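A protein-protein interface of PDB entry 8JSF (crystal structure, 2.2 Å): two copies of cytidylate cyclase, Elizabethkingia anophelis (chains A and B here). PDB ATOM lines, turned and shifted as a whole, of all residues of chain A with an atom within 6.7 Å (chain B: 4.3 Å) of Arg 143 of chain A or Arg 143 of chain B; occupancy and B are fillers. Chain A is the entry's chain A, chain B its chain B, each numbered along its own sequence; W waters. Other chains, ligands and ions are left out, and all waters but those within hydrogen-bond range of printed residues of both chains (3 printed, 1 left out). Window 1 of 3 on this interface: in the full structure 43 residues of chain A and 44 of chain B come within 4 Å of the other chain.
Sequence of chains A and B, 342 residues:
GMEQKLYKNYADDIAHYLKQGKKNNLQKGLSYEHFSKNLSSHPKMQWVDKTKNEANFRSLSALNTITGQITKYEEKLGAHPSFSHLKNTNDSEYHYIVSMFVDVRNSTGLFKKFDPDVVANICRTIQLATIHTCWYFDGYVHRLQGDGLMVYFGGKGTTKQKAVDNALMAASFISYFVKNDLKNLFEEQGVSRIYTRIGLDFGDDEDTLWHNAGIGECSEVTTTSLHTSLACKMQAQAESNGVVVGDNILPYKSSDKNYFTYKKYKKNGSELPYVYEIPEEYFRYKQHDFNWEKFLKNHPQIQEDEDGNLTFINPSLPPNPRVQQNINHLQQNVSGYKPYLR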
ATOM      1  N   LEU A  77     -19.955  15.206 -20.077  1.00  0.00           N
ATOM      2  CA  LEU A  77     -19.723  13.971 -20.804  1.00  0.00           C
ATOM      3  C   LEU A  77     -21.044  13.249 -21.058  1.00  0.00           C
ATOM      4  O   LEU A  77     -22.057  13.504 -20.399  1.00  0.00           O
ATOM      5  CB  LEU A  77     -18.766  13.063 -20.028  1.00  0.00           C
ATOM      6  CG  LEU A  77     -17.388  13.661 -19.721  1.00  0.00           C
ATOM      7  CD1 LEU A  77     -16.636  12.816 -18.693  1.00  0.00           C
ATOM      8  CD2 LEU A  77     -16.576  13.814 -20.997  1.00  0.00           C
ATOM      9  N   GLY A  78     -21.033  12.376 -22.064  1.00  0.00           N
ATOM     10  CA  GLY A  78     -22.200  11.559 -22.364  1.00  0.00           C
ATOM     11  C   GLY A  78     -23.425  12.345 -22.769  1.00  0.00           C
ATOM     12  O   GLY A  78     -24.550  11.891 -22.533  1.00  0.00           O
ATOM     13  N   PHE A 101     -11.892   7.609 -31.762  1.00  0.00           N
ATOM     14  CA  PHE A 101     -11.396   6.976 -30.549  1.00  0.00           C
ATOM     15  C   PHE A 101      -9.898   7.227 -30.456  1.00  0.00           C
ATOM     16  O   PHE A 101      -9.158   6.936 -31.403  1.00  0.00           O
ATOM     17  CB  PHE A 101     -11.693   5.475 -30.547  1.00  0.00           C
ATOM     18  CG  PHE A 101     -13.136   5.135 -30.274  1.00  0.00           C
ATOM     19  CD1 PHE A 101     -14.098   5.281 -31.262  1.00  0.00           C
ATOM     20  CD2 PHE A 101     -13.524   4.637 -29.036  1.00  0.00           C
ATOM     21  CE1 PHE A 101     -15.424   4.960 -31.016  1.00  0.00           C
ATOM     22  CE2 PHE A 101     -14.846   4.309 -28.783  1.00  0.00           C
ATOM     23  CZ  PHE A 101     -15.797   4.474 -29.772  1.00  0.00           C
ATOM     24  N   GLN A 127      -3.915  14.073 -21.418  1.00  0.00           N
ATOM     25  CA  GLN A 127      -5.345  14.072 -21.696  1.00  0.00           C
ATOM     26  C   GLN A 127      -5.883  15.490 -21.853  1.00  0.00           C
ATOM     27  O   GLN A 127      -6.735  15.737 -22.711  1.00  0.00           O
ATOM     28  CB  GLN A 127      -6.081  13.300 -20.602  1.00  0.00           C
ATOM     29  CG  GLN A 127      -7.579  13.223 -20.785  1.00  0.00           C
ATOM     30  CD  GLN A 127      -8.229  12.307 -19.769  1.00  0.00           C
ATOM     31  OE1 GLN A 127      -8.327  12.635 -18.589  1.00  0.00           O
ATOM     32  NE2 GLN A 127      -8.671  11.140 -20.229  1.00  0.00           N
ATOM     33  N   TYR A 140     -16.745  17.398 -29.772  1.00  0.00           N
ATOM     34  CA  TYR A 140     -17.420  17.164 -28.504  1.00  0.00           C
ATOM     35  C   TYR A 140     -16.797  15.945 -27.836  1.00  0.00           C
ATOM     36  O   TYR A 140     -16.841  14.839 -28.388  1.00  0.00           O
ATOM     37  CB  TYR A 140     -18.920  16.946 -28.693  1.00  0.00           C
ATOM     38  CG  TYR A 140     -19.542  16.364 -27.442  1.00  0.00           C
ATOM     39  CD1 TYR A 140     -19.684  17.139 -26.299  1.00  0.00           C
ATOM     40  CD2 TYR A 140     -19.959  15.037 -27.390  1.00  0.00           C
ATOM     41  CE1 TYR A 140     -20.231  16.619 -25.142  1.00  0.00           C
ATOM     42  CE2 TYR A 140     -20.512  14.508 -26.231  1.00  0.00           C
ATOM     43  CZ  TYR A 140     -20.644  15.307 -25.110  1.00  0.00           C
ATOM     44  OH  TYR A 140     -21.183  14.797 -23.950  1.00  0.00           O
ATOM     45  N   VAL A 141     -16.234  16.143 -26.646  1.00  0.00           N
ATOM     46  CA  VAL A 141     -15.648  15.050 -25.874  1.00  0.00           C
ATOM     47  C   VAL A 141     -16.782  14.296 -25.187  1.00  0.00           C
ATOM     48  O   VAL A 141     -17.418  14.811 -24.265  1.00  0.00           O
ATOM     49  CB  VAL A 141     -14.625  15.569 -24.858  1.00  0.00           C
ATOM     50  CG1 VAL A 141     -14.045  14.427 -24.053  1.00  0.00           C
ATOM     51  CG2 VAL A 141     -13.516  16.323 -25.577  1.00  0.00           C
ATOM     52  N   HIS A 142     -17.043  13.074 -25.643  1.00  0.00           N
ATOM     53  CA  HIS A 142     -18.160  12.278 -25.164  1.00  0.00           C
ATOM     54  C   HIS A 142     -17.806  11.468 -23.923  1.00  0.00           C
ATOM     55  O   HIS A 142     -18.629  11.337 -23.008  1.00  0.00           O
ATOM     56  CB  HIS A 142     -18.630  11.349 -26.291  1.00  0.00           C
ATOM     57  CG  HIS A 142     -19.693  10.380 -25.880  1.00  0.00           C
ATOM     58  ND1 HIS A 142     -20.987  10.765 -25.607  1.00  0.00           N
ATOM     59  CD2 HIS A 142     -19.656   9.037 -25.708  1.00  0.00           C
ATOM     60  CE1 HIS A 142     -21.700   9.703 -25.277  1.00  0.00           C
ATOM     61  NE2 HIS A 142     -20.916   8.642 -25.328  1.00  0.00           N
ATOM     62  N   ARG A 143     -16.588  10.935 -23.863  1.00  0.00           N
ATOM     63  CA  ARG A 143     -16.226  10.004 -22.810  1.00  0.00           C
ATOM     64  C   ARG A 143     -14.734  10.109 -22.531  1.00  0.00           C
ATOM     65  O   ARG A 143     -13.930  10.250 -23.456  1.00  0.00           O
ATOM     66  CB  ARG A 143     -16.590   8.564 -23.207  1.00  0.00           C
ATOM     67  CG  ARG A 143     -16.499   7.562 -22.072  1.00  0.00           C
ATOM     68  CD  ARG A 143     -16.821   6.140 -22.543  1.00  0.00           C
ATOM     69  NE  ARG A 143     -18.140   6.020 -23.160  1.00  0.00           N
ATOM     70  CZ  ARG A 143     -18.350   5.537 -24.378  1.00  0.00           C
ATOM     71  NH1 ARG A 143     -17.349   5.137 -25.144  1.00  0.00           N
ATOM     72  NH2 ARG A 143     -19.597   5.431 -24.829  1.00  0.00           N
ATOM     73  N   LEU A 144     -14.372  10.024 -21.257  1.00  0.00           N
ATOM     74  CA  LEU A 144     -12.980   9.947 -20.842  1.00  0.00           C
ATOM     75  C   LEU A 144     -12.667   8.503 -20.468  1.00  0.00           C
ATOM     76  O   LEU A 144     -13.319   7.932 -19.588  1.00  0.00           O
ATOM     77  CB  LEU A 144     -12.694  10.864 -19.651  1.00  0.00           C
ATOM     78  CG  LEU A 144     -13.002  12.361 -19.724  1.00  0.00           C
ATOM     79  CD1 LEU A 144     -12.510  13.053 -18.458  1.00  0.00           C
ATOM     80  CD2 LEU A 144     -12.382  12.994 -20.939  1.00  0.00           C
ATOM     81  N   GLN A 145     -11.697   7.911 -21.153  1.00  0.00           N
ATOM     82  CA  GLN A 145     -11.081   6.686 -20.671  1.00  0.00           C
ATOM     83  C   GLN A 145      -9.920   7.027 -19.742  1.00  0.00           C
ATOM     84  O   GLN A 145      -9.482   8.176 -19.638  1.00  0.00           O
ATOM     85  CB  GLN A 145     -10.574   5.835 -21.836  1.00  0.00           C
ATOM     86  CG  GLN A 145     -11.621   5.012 -22.579  1.00  0.00           C
ATOM     87  CD  GLN A 145     -12.584   5.833 -23.420  1.00  0.00           C
ATOM     88  OE1 GLN A 145     -12.455   7.052 -23.521  1.00  0.00           O
ATOM     89  NE2 GLN A 145     -13.557   5.157 -24.037  1.00  0.00           N
ATOM     90  N   GLY A 146      -9.401   6.008 -19.068  1.00  0.00           N
ATOM     91  CA  GLY A 146      -8.152   6.198 -18.356  1.00  0.00           C
ATOM     92  C   GLY A 146      -7.008   6.464 -19.314  1.00  0.00           C
ATOM     93  O   GLY A 146      -6.157   7.322 -19.063  1.00  0.00           O
ATOM     94  N   ASP A 147      -6.990   5.748 -20.434  1.00  0.00           N
ATOM     95  CA  ASP A 147      -5.937   5.839 -21.436  1.00  0.00           C
ATOM     96  C   ASP A 147      -6.454   6.347 -22.782  1.00  0.00           C
ATOM     97  O   ASP A 147      -6.003   5.894 -23.836  1.00  0.00           O
ATOM     98  CB  ASP A 147      -5.256   4.484 -21.604  1.00  0.00           C
ATOM     99  CG  ASP A 147      -6.251   3.354 -21.824  1.00  0.00           C
ATOM    100  OD1 ASP A 147      -7.473   3.626 -21.840  1.00  0.00           O
ATOM    101  OD2 ASP A 147      -5.814   2.191 -21.968  1.00  0.00           O
ATOM    102  N   GLY A 148      -7.400   7.278 -22.781  1.00  0.00           N
ATOM    103  CA  GLY A 148      -7.837   7.861 -24.033  1.00  0.00           C
ATOM    104  C   GLY A 148      -9.163   8.587 -23.915  1.00  0.00           C
ATOM    105  O   GLY A 148      -9.667   8.842 -22.823  1.00  0.00           O
ATOM    106  N   LEU A 149      -9.698   8.931 -25.086  1.00  0.00           N
ATOM    107  CA  LEU A 149     -10.935   9.691 -25.220  1.00  0.00           C
ATOM    108  C   LEU A 149     -11.816   9.095 -26.307  1.00  0.00           C
ATOM    109  O   LEU A 149     -11.344   8.435 -27.236  1.00  0.00           O
ATOM    110  CB  LEU A 149     -10.705  11.167 -25.594  1.00  0.00           C
ATOM    111  CG  LEU A 149      -9.769  12.099 -24.844  1.00  0.00           C
ATOM    112  CD1 LEU A 149      -9.951  13.498 -25.380  1.00  0.00           C
ATOM    113  CD2 LEU A 149     -10.091  12.060 -23.375  1.00  0.00           C
ATOM    114  N   MET A 150     -13.110   9.369 -26.190  1.00  0.00           N
ATOM    115  CA  MET A 150     -14.065   9.160 -27.266  1.00  0.00           C
ATOM    116  C   MET A 150     -14.636  10.525 -27.623  1.00  0.00           C
ATOM    117  O   MET A 150     -15.123  11.243 -26.743  1.00  0.00           O
ATOM    118  CB  MET A 150     -15.170   8.182 -26.850  1.00  0.00           C
ATOM    119  CG  MET A 150     -15.946   7.583 -28.015  1.00  0.00           C
ATOM    120  SD  MET A 150     -17.191   8.708 -28.672  1.00  0.00           S
ATOM    121  CE  MET A 150     -17.050   8.389 -30.435  1.00  0.00           C
ATOM    122  N   VAL A 151     -14.543  10.893 -28.901  1.00  0.00           N
ATOM    123  CA  VAL A 151     -14.880  12.231 -29.373  1.00  0.00           C
ATOM    124  C   VAL A 151     -15.817  12.124 -30.568  1.00  0.00           C
ATOM    125  O   VAL A 151     -15.634  11.269 -31.441  1.00  0.00           O
ATOM    126  CB  VAL A 151     -13.613  13.031 -29.753  1.00  0.00           C
ATOM    127  CG1 VAL A 151     -13.962  14.479 -30.087  1.00  0.00           C
ATOM    128  CG2 VAL A 151     -12.584  12.973 -28.625  1.00  0.00           C
ATOM    129  N   TYR A 152     -16.828  12.985 -30.605  1.00  0.00           N
ATOM    130  CA  TYR A 152     -17.692  13.125 -31.768  1.00  0.00           C
ATOM    131  C   TYR A 152     -17.355  14.419 -32.493  1.00  0.00           C
ATOM    132  O   TYR A 152     -17.045  15.435 -31.865  1.00  0.00           O
ATOM    133  CB  TYR A 152     -19.174  13.122 -31.378  1.00  0.00           C
ATOM    134  CG  TYR A 152     -19.740  11.772 -30.965  1.00  0.00           C
ATOM    135  CD1 TYR A 152     -19.787  10.706 -31.855  1.00  0.00           C
ATOM    136  CD2 TYR A 152     -20.249  11.577 -29.686  1.00  0.00           C
ATOM    137  CE1 TYR A 152     -20.319   9.478 -31.477  1.00  0.00           C
ATOM    138  CE2 TYR A 152     -20.777  10.359 -29.301  1.00  0.00           C
ATOM    139  CZ  TYR A 152     -20.811   9.314 -30.198  1.00  0.00           C
ATOM    140  OH  TYR A 152     -21.340   8.106 -29.806  1.00  0.00           O
ATOM    141  N   CYS A 218     -26.929   6.602 -14.153  1.00  0.00           N
ATOM    142  CA  CYS A 218     -25.983   5.671 -14.764  1.00  0.00           C
ATOM    143  C   CYS A 218     -26.392   5.481 -16.223  1.00  0.00           C
ATOM    144  O   CYS A 218     -26.882   4.432 -16.645  1.00  0.00           O
ATOM    145  CB  CYS A 218     -25.968   4.352 -14.004  1.00  0.00           C
ATOM    146  SG  CYS A 218     -24.783   3.141 -14.634  1.00  0.00           S
ATOM    147  N   GLU A 220     -26.193   7.547 -20.473  1.00  0.00           N
ATOM    148  CA  GLU A 220     -25.629   8.519 -21.398  1.00  0.00           C
ATOM    149  C   GLU A 220     -26.515   8.617 -22.632  1.00  0.00           C
ATOM    150  O   GLU A 220     -27.338   7.739 -22.906  1.00  0.00           O
ATOM    151  CB  GLU A 220     -24.185   8.150 -21.786  1.00  0.00           C
ATOM    152  CG  GLU A 220     -24.055   6.793 -22.461  1.00  0.00           C
ATOM    153  CD  GLU A 220     -22.621   6.437 -22.838  1.00  0.00           C
ATOM    154  OE1 GLU A 220     -21.677   7.108 -22.362  1.00  0.00           O
ATOM    155  OE2 GLU A 220     -22.444   5.466 -23.603  1.00  0.00           O
ATOM    156  N   THR A 222     -25.920   8.492 -26.475  1.00  0.00           N
ATOM    157  CA  THR A 222     -24.811   7.963 -27.254  1.00  0.00           C
ATOM    158  C   THR A 222     -25.343   7.461 -28.591  1.00  0.00           C
ATOM    159  O   THR A 222     -26.537   7.570 -28.889  1.00  0.00           O
ATOM    160  CB  THR A 222     -24.078   6.866 -26.472  1.00  0.00           C
ATOM    161  OG1 THR A 222     -22.855   6.533 -27.137  1.00  0.00           O
ATOM    162  CG2 THR A 222     -24.948   5.616 -26.343  1.00  0.00           C
ATOM    163  N   LEU B  77     -22.141   8.779 -13.393  1.00  0.00           N
ATOM    164  CA  LEU B  77     -20.908   8.172 -13.860  1.00  0.00           C
ATOM    165  C   LEU B  77     -19.730   9.077 -13.522  1.00  0.00           C
ATOM    166  O   LEU B  77     -19.875  10.294 -13.386  1.00  0.00           O
ATOM    167  CB  LEU B  77     -20.982   7.950 -15.368  1.00  0.00           C
ATOM    168  CG  LEU B  77     -22.132   7.046 -15.832  1.00  0.00           C
ATOM    169  CD1 LEU B  77     -22.342   7.165 -17.333  1.00  0.00           C
ATOM    170  CD2 LEU B  77     -21.836   5.602 -15.452  1.00  0.00           C
ATOM    171  N   VAL B 141     -21.004   1.726 -10.724  1.00  0.00           N
ATOM    172  CA  VAL B 141     -20.722   1.770 -12.157  1.00  0.00           C
ATOM    173  C   VAL B 141     -20.088   3.118 -12.486  1.00  0.00           C
ATOM    174  O   VAL B 141     -20.744   4.160 -12.414  1.00  0.00           O
ATOM    175  CB  VAL B 141     -21.985   1.524 -12.991  1.00  0.00           C
ATOM    176  CG1 VAL B 141     -21.646   1.557 -14.464  1.00  0.00           C
ATOM    177  CG2 VAL B 141     -22.604   0.166 -12.626  1.00  0.00           C
ATOM    178  N   HIS B 142     -18.804   3.096 -12.840  1.00  0.00           N
ATOM    179  CA  HIS B 142     -17.990   4.281 -13.082  1.00  0.00           C
ATOM    180  C   HIS B 142     -18.085   4.785 -14.516  1.00  0.00           C
ATOM    181  O   HIS B 142     -18.086   6.001 -14.745  1.00  0.00           O
ATOM    182  CB  HIS B 142     -16.535   3.954 -12.732  1.00  0.00           C
ATOM    183  CG  HIS B 142     -15.557   5.024 -13.097  1.00  0.00           C
ATOM    184  ND1 HIS B 142     -15.492   6.233 -12.438  1.00  0.00           N
ATOM    185  CD2 HIS B 142     -14.575   5.047 -14.029  1.00  0.00           C
ATOM    186  CE1 HIS B 142     -14.523   6.964 -12.963  1.00  0.00           C
ATOM    187  NE2 HIS B 142     -13.952   6.268 -13.931  1.00  0.00           N
ATOM    188  N   ARG B 143     -18.157   3.878 -15.491  1.00  0.00           N
ATOM    189  CA  ARG B 143     -18.101   4.268 -16.892  1.00  0.00           C
ATOM    190  C   ARG B 143     -18.894   3.274 -17.725  1.00  0.00           C
ATOM    191  O   ARG B 143     -18.849   2.068 -17.469  1.00  0.00           O
ATOM    192  CB  ARG B 143     -16.645   4.337 -17.378  1.00  0.00           C
ATOM    193  CG  ARG B 143     -16.462   4.972 -18.748  1.00  0.00           C
ATOM    194  CD  ARG B 143     -14.986   4.992 -19.156  1.00  0.00           C
ATOM    195  NE  ARG B 143     -14.167   5.716 -18.188  1.00  0.00           N
ATOM    196  CZ  ARG B 143     -13.107   5.210 -17.572  1.00  0.00           C
ATOM    197  NH1 ARG B 143     -12.706   3.965 -17.794  1.00  0.00           N
ATOM    198  NH2 ARG B 143     -12.430   5.970 -16.716  1.00  0.00           N
ATOM    199  N   LEU B 144     -19.637   3.794 -18.701  1.00  0.00           N
ATOM    200  CA  LEU B 144     -20.338   2.992 -19.698  1.00  0.00           C
ATOM    201  C   LEU B 144     -19.617   3.115 -21.033  1.00  0.00           C
ATOM    202  O   LEU B 144     -19.481   4.221 -21.564  1.00  0.00           O
ATOM    203  CB  LEU B 144     -21.792   3.440 -19.857  1.00  0.00           C
ATOM    204  CG  LEU B 144     -22.731   3.493 -18.655  1.00  0.00           C
ATOM    205  CD1 LEU B 144     -24.136   3.858 -19.110  1.00  0.00           C
ATOM    206  CD2 LEU B 144     -22.747   2.172 -17.928  1.00  0.00           C
ATOM    207  N   GLN B 145     -19.140   1.992 -21.562  1.00  0.00           N
ATOM    208  CA  GLN B 145     -18.744   1.919 -22.960  1.00  0.00           C
ATOM    209  C   GLN B 145     -19.919   1.460 -23.815  1.00  0.00           C
ATOM    210  O   GLN B 145     -20.967   1.043 -23.319  1.00  0.00           O
ATOM    211  CB  GLN B 145     -17.570   0.963 -23.165  1.00  0.00           C
ATOM    212  CG  GLN B 145     -16.222   1.505 -22.754  1.00  0.00           C
ATOM    213  CD  GLN B 145     -16.047   1.582 -21.251  1.00  0.00           C
ATOM    214  OE1 GLN B 145     -16.910   1.147 -20.490  1.00  0.00           O
ATOM    215  NE2 GLN B 145     -14.927   2.141 -20.815  1.00  0.00           N
ATOM    216  N   GLY B 146     -19.719   1.510 -25.129  1.00  0.00           N
ATOM    217  CA  GLY B 146     -20.667   0.867 -26.018  1.00  0.00           C
ATOM    218  C   GLY B 146     -20.685  -0.636 -25.818  1.00  0.00           C
ATOM    219  O   GLY B 146     -21.746  -1.264 -25.855  1.00  0.00           O
ATOM    220  N   LEU B 149     -18.472  -2.113 -19.437  1.00  0.00           N
ATOM    221  CA  LEU B 149     -18.569  -1.263 -18.259  1.00  0.00           C
ATOM    222  C   LEU B 149     -17.259  -1.289 -17.492  1.00  0.00           C
ATOM    223  O   LEU B 149     -16.496  -2.256 -17.554  1.00  0.00           O
ATOM    224  CB  LEU B 149     -19.663  -1.712 -17.277  1.00  0.00           C
ATOM    225  CG  LEU B 149     -21.084  -2.045 -17.692  1.00  0.00           C
ATOM    226  CD1 LEU B 149     -21.929  -2.202 -16.439  1.00  0.00           C
ATOM    227  CD2 LEU B 149     -21.639  -0.990 -18.598  1.00  0.00           C
ATOM    228  N   MET B 150     -17.037  -0.227 -16.723  1.00  0.00           N
ATOM    229  CA  MET B 150     -16.003  -0.181 -15.699  1.00  0.00           C
ATOM    230  C   MET B 150     -16.696  -0.003 -14.354  1.00  0.00           C
ATOM    231  O   MET B 150     -17.505   0.915 -14.189  1.00  0.00           O
ATOM    232  CB  MET B 150     -15.008   0.953 -15.965  1.00  0.00           C
ATOM    233  CG  MET B 150     -13.690   0.835 -15.194  1.00  0.00           C
ATOM    234  SD  MET B 150     -13.799   1.394 -13.481  1.00  0.00           S
ATOM    235  CE  MET B 150     -12.757   0.192 -12.645  1.00  0.00           C
ATOM    236  N   GLU B 220     -14.044  13.659 -14.793  1.00  0.00           N
ATOM    237  CA  GLU B 220     -14.513  12.562 -13.962  1.00  0.00           C
ATOM    238  C   GLU B 220     -13.589  12.460 -12.762  1.00  0.00           C
ATOM    239  O   GLU B 220     -12.420  12.835 -12.833  1.00  0.00           O
ATOM    240  CB  GLU B 220     -14.546  11.222 -14.722  1.00  0.00           C
ATOM    241  CG  GLU B 220     -13.194  10.742 -15.231  1.00  0.00           C
ATOM    242  CD  GLU B 220     -13.269   9.399 -15.958  1.00  0.00           C
ATOM    243  OE1 GLU B 220     -14.383   8.952 -16.311  1.00  0.00           O
ATOM    244  OE2 GLU B 220     -12.205   8.787 -16.173  1.00  0.00           O
ATOM    245  N   THR B 222     -11.620   9.730 -10.780  1.00  0.00           N
ATOM    246  CA  THR B 222     -11.180   8.400 -11.171  1.00  0.00           C
ATOM    247  C   THR B 222      -9.926   8.050 -10.381  1.00  0.00           C
ATOM    248  O   THR B 222      -9.455   8.828  -9.544  1.00  0.00           O
ATOM    249  CB  THR B 222     -10.941   8.332 -12.688  1.00  0.00           C
ATOM    250  OG1 THR B 222     -10.744   6.968 -13.087  1.00  0.00           O
ATOM    251  CG2 THR B 222      -9.716   9.149 -13.080  1.00  0.00           C
HETATM  252  O   HOH W   1      -9.974   9.438 -17.190  1.00  0.00           O
HETATM  253  O   HOH W   2     -18.515   3.442 -27.180  1.00  0.00           O
HETATM  254  O   HOH W   3     -23.380   5.001 -11.862  1.00  0.00           O
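The backbone carbonyl oxygen (O) of Leu 144 of chain B sits at hydrogen-bond distance from the guanidinium group (NE) of Arg 143 of chain A (2.8 Å).
O of Leu 144 of chain A is in hydrogen-bond range of NE of Arg 143 of chain B, 2.8 Å away.
NE2 of His 142 of chain A lies within hydrogen-bond range of OE1 of Glu 220 of chain A, at 3.4 Å.
The guanidinium group of Arg 143 of chain A is in salt-bridge range of the side-chain carboxylate of Glu 220 of chain A (3.1 Å).
The side-chain amide oxygen (OE1) of Gln 145 of chain A sits close to the backbone carbonyl oxygen (O) of Gly 148 of chain A (3.4 Å).
NE2 of His 142 of chain B lies within hydrogen-bond range of NH2 of Arg 143 of chain B (3.2 Å).
The backbone NH (N) of Met 150 of chain B is in hydrogen-bond range of the backbone carbonyl oxygen (O) of Arg 143 of chain B, at 3.0 Å.
NH2 of Arg 143 of chain B is in salt-bridge range of OE2 of Glu 220 of chain B.
Among the printed residues, pairs that only touch across the chains: Cys 218 of chain A with Val 141 of chain B, Leu 144 of chain A with Glu 220 of chain B, Glu 220 of chain A with Leu 144 of chain B, Cys 218 of chain A with Leu 144 of chain B, Gly 146 of chain A with Arg 143 of chain B, Arg 143 of chain A with Gln 145 of chain B, Cys 218 of chain A with Leu 77 of chain B, Arg 143 of chain A with Gly 146 of chain B, Gln 145 of chain A with Arg 143 of chain B and Arg 143 of chain A with Arg 143 of chain B.
Of the printed residues of chain B, Arg 143 of chain A touches Arg 143 (3.99 Å), Leu 144 (2.8 Å), Gln 145 (3.9 Å) and Gly 146 (3.9 Å).
Of the printed residues of chain A, Arg 143 of chain B touches Arg 143, Leu 144, Gln 145 and Gly 146.
Printed residues of chain A within 4 Å of Glu 220 of chain B: Leu 144 (3.6 Å).
Printed residues of chain B within 4 Å of Cys 218 of chain A: Leu 77, Val 141 and Leu 144.
Printed residues of chain A within 4 Å of Gly 146 of chain B: Arg 143.
Of the printed residues of chain B, Gln 145 of chain A touches Arg 143 (3.99 Å).
Met 150 of chain A touches none of the printed residues of chain B.
The nearest printed residue of chain A that does not touch Arg 143 of chain B is Asp 147 of chain A (6.5 Å).
The nearest printed residue of chain B that does not touch Gln 145 of chain A is Glu 220 of chain B (4.4 Å).
Of the 11 printed residues of chain B, 7 touch a printed residue of chain A.
Hydrophobic or aromatic side chains of chain B within 4 Å of the printed part of chain A: Leu 77, Val 141 and Leu 144.
Of the 20 printed residues of chain A, 6 touch a printed residue of chain B.
Among the printed residues, 12 pairs touch across the chains.
Among the printed residues, no Asp or Glu carboxylate lies within 4 Å of a Lys or Arg side-chain nitrogen of the other chain.
Arg 143 of chain B touches its own counterpart, Arg 143 of chain A.
Arg 143 of chain A touches Leu 144 of chain B, and with the chains exchanged Leu 144 of chain A touches Arg 143 of chain B.
Arg 143 of chain A touches Gly 146 of chain B, and with the chains exchanged Gly 146 of chain A touches Arg 143 of chain B.
Leu 144 of chain A touches Glu 220 of chain B, and with the chains exchanged Glu 220 of chain A touches Leu 144 of chain B.
11 positions are printed for both chains.
Of the 12 pairs that touch across the chains among the printed residues, 9 have their exchanged pair printed and touching as well.
Water W1 lies within hydrogen-bond range of the side-chain carboxylate of Glu 220 of chain B (2.5 Å) and the backbone carbonyl oxygen of Gln 145 of chain A (2.8 Å).
Water W3 bridges O of Val 141 of chain B and SG of Cys 218 of chain A.
Water W2 lies within hydrogen-bond range of NH1 of Arg 143 of chain A (2.9 Å) and N of Gly 146 of chain B (3.1 Å).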
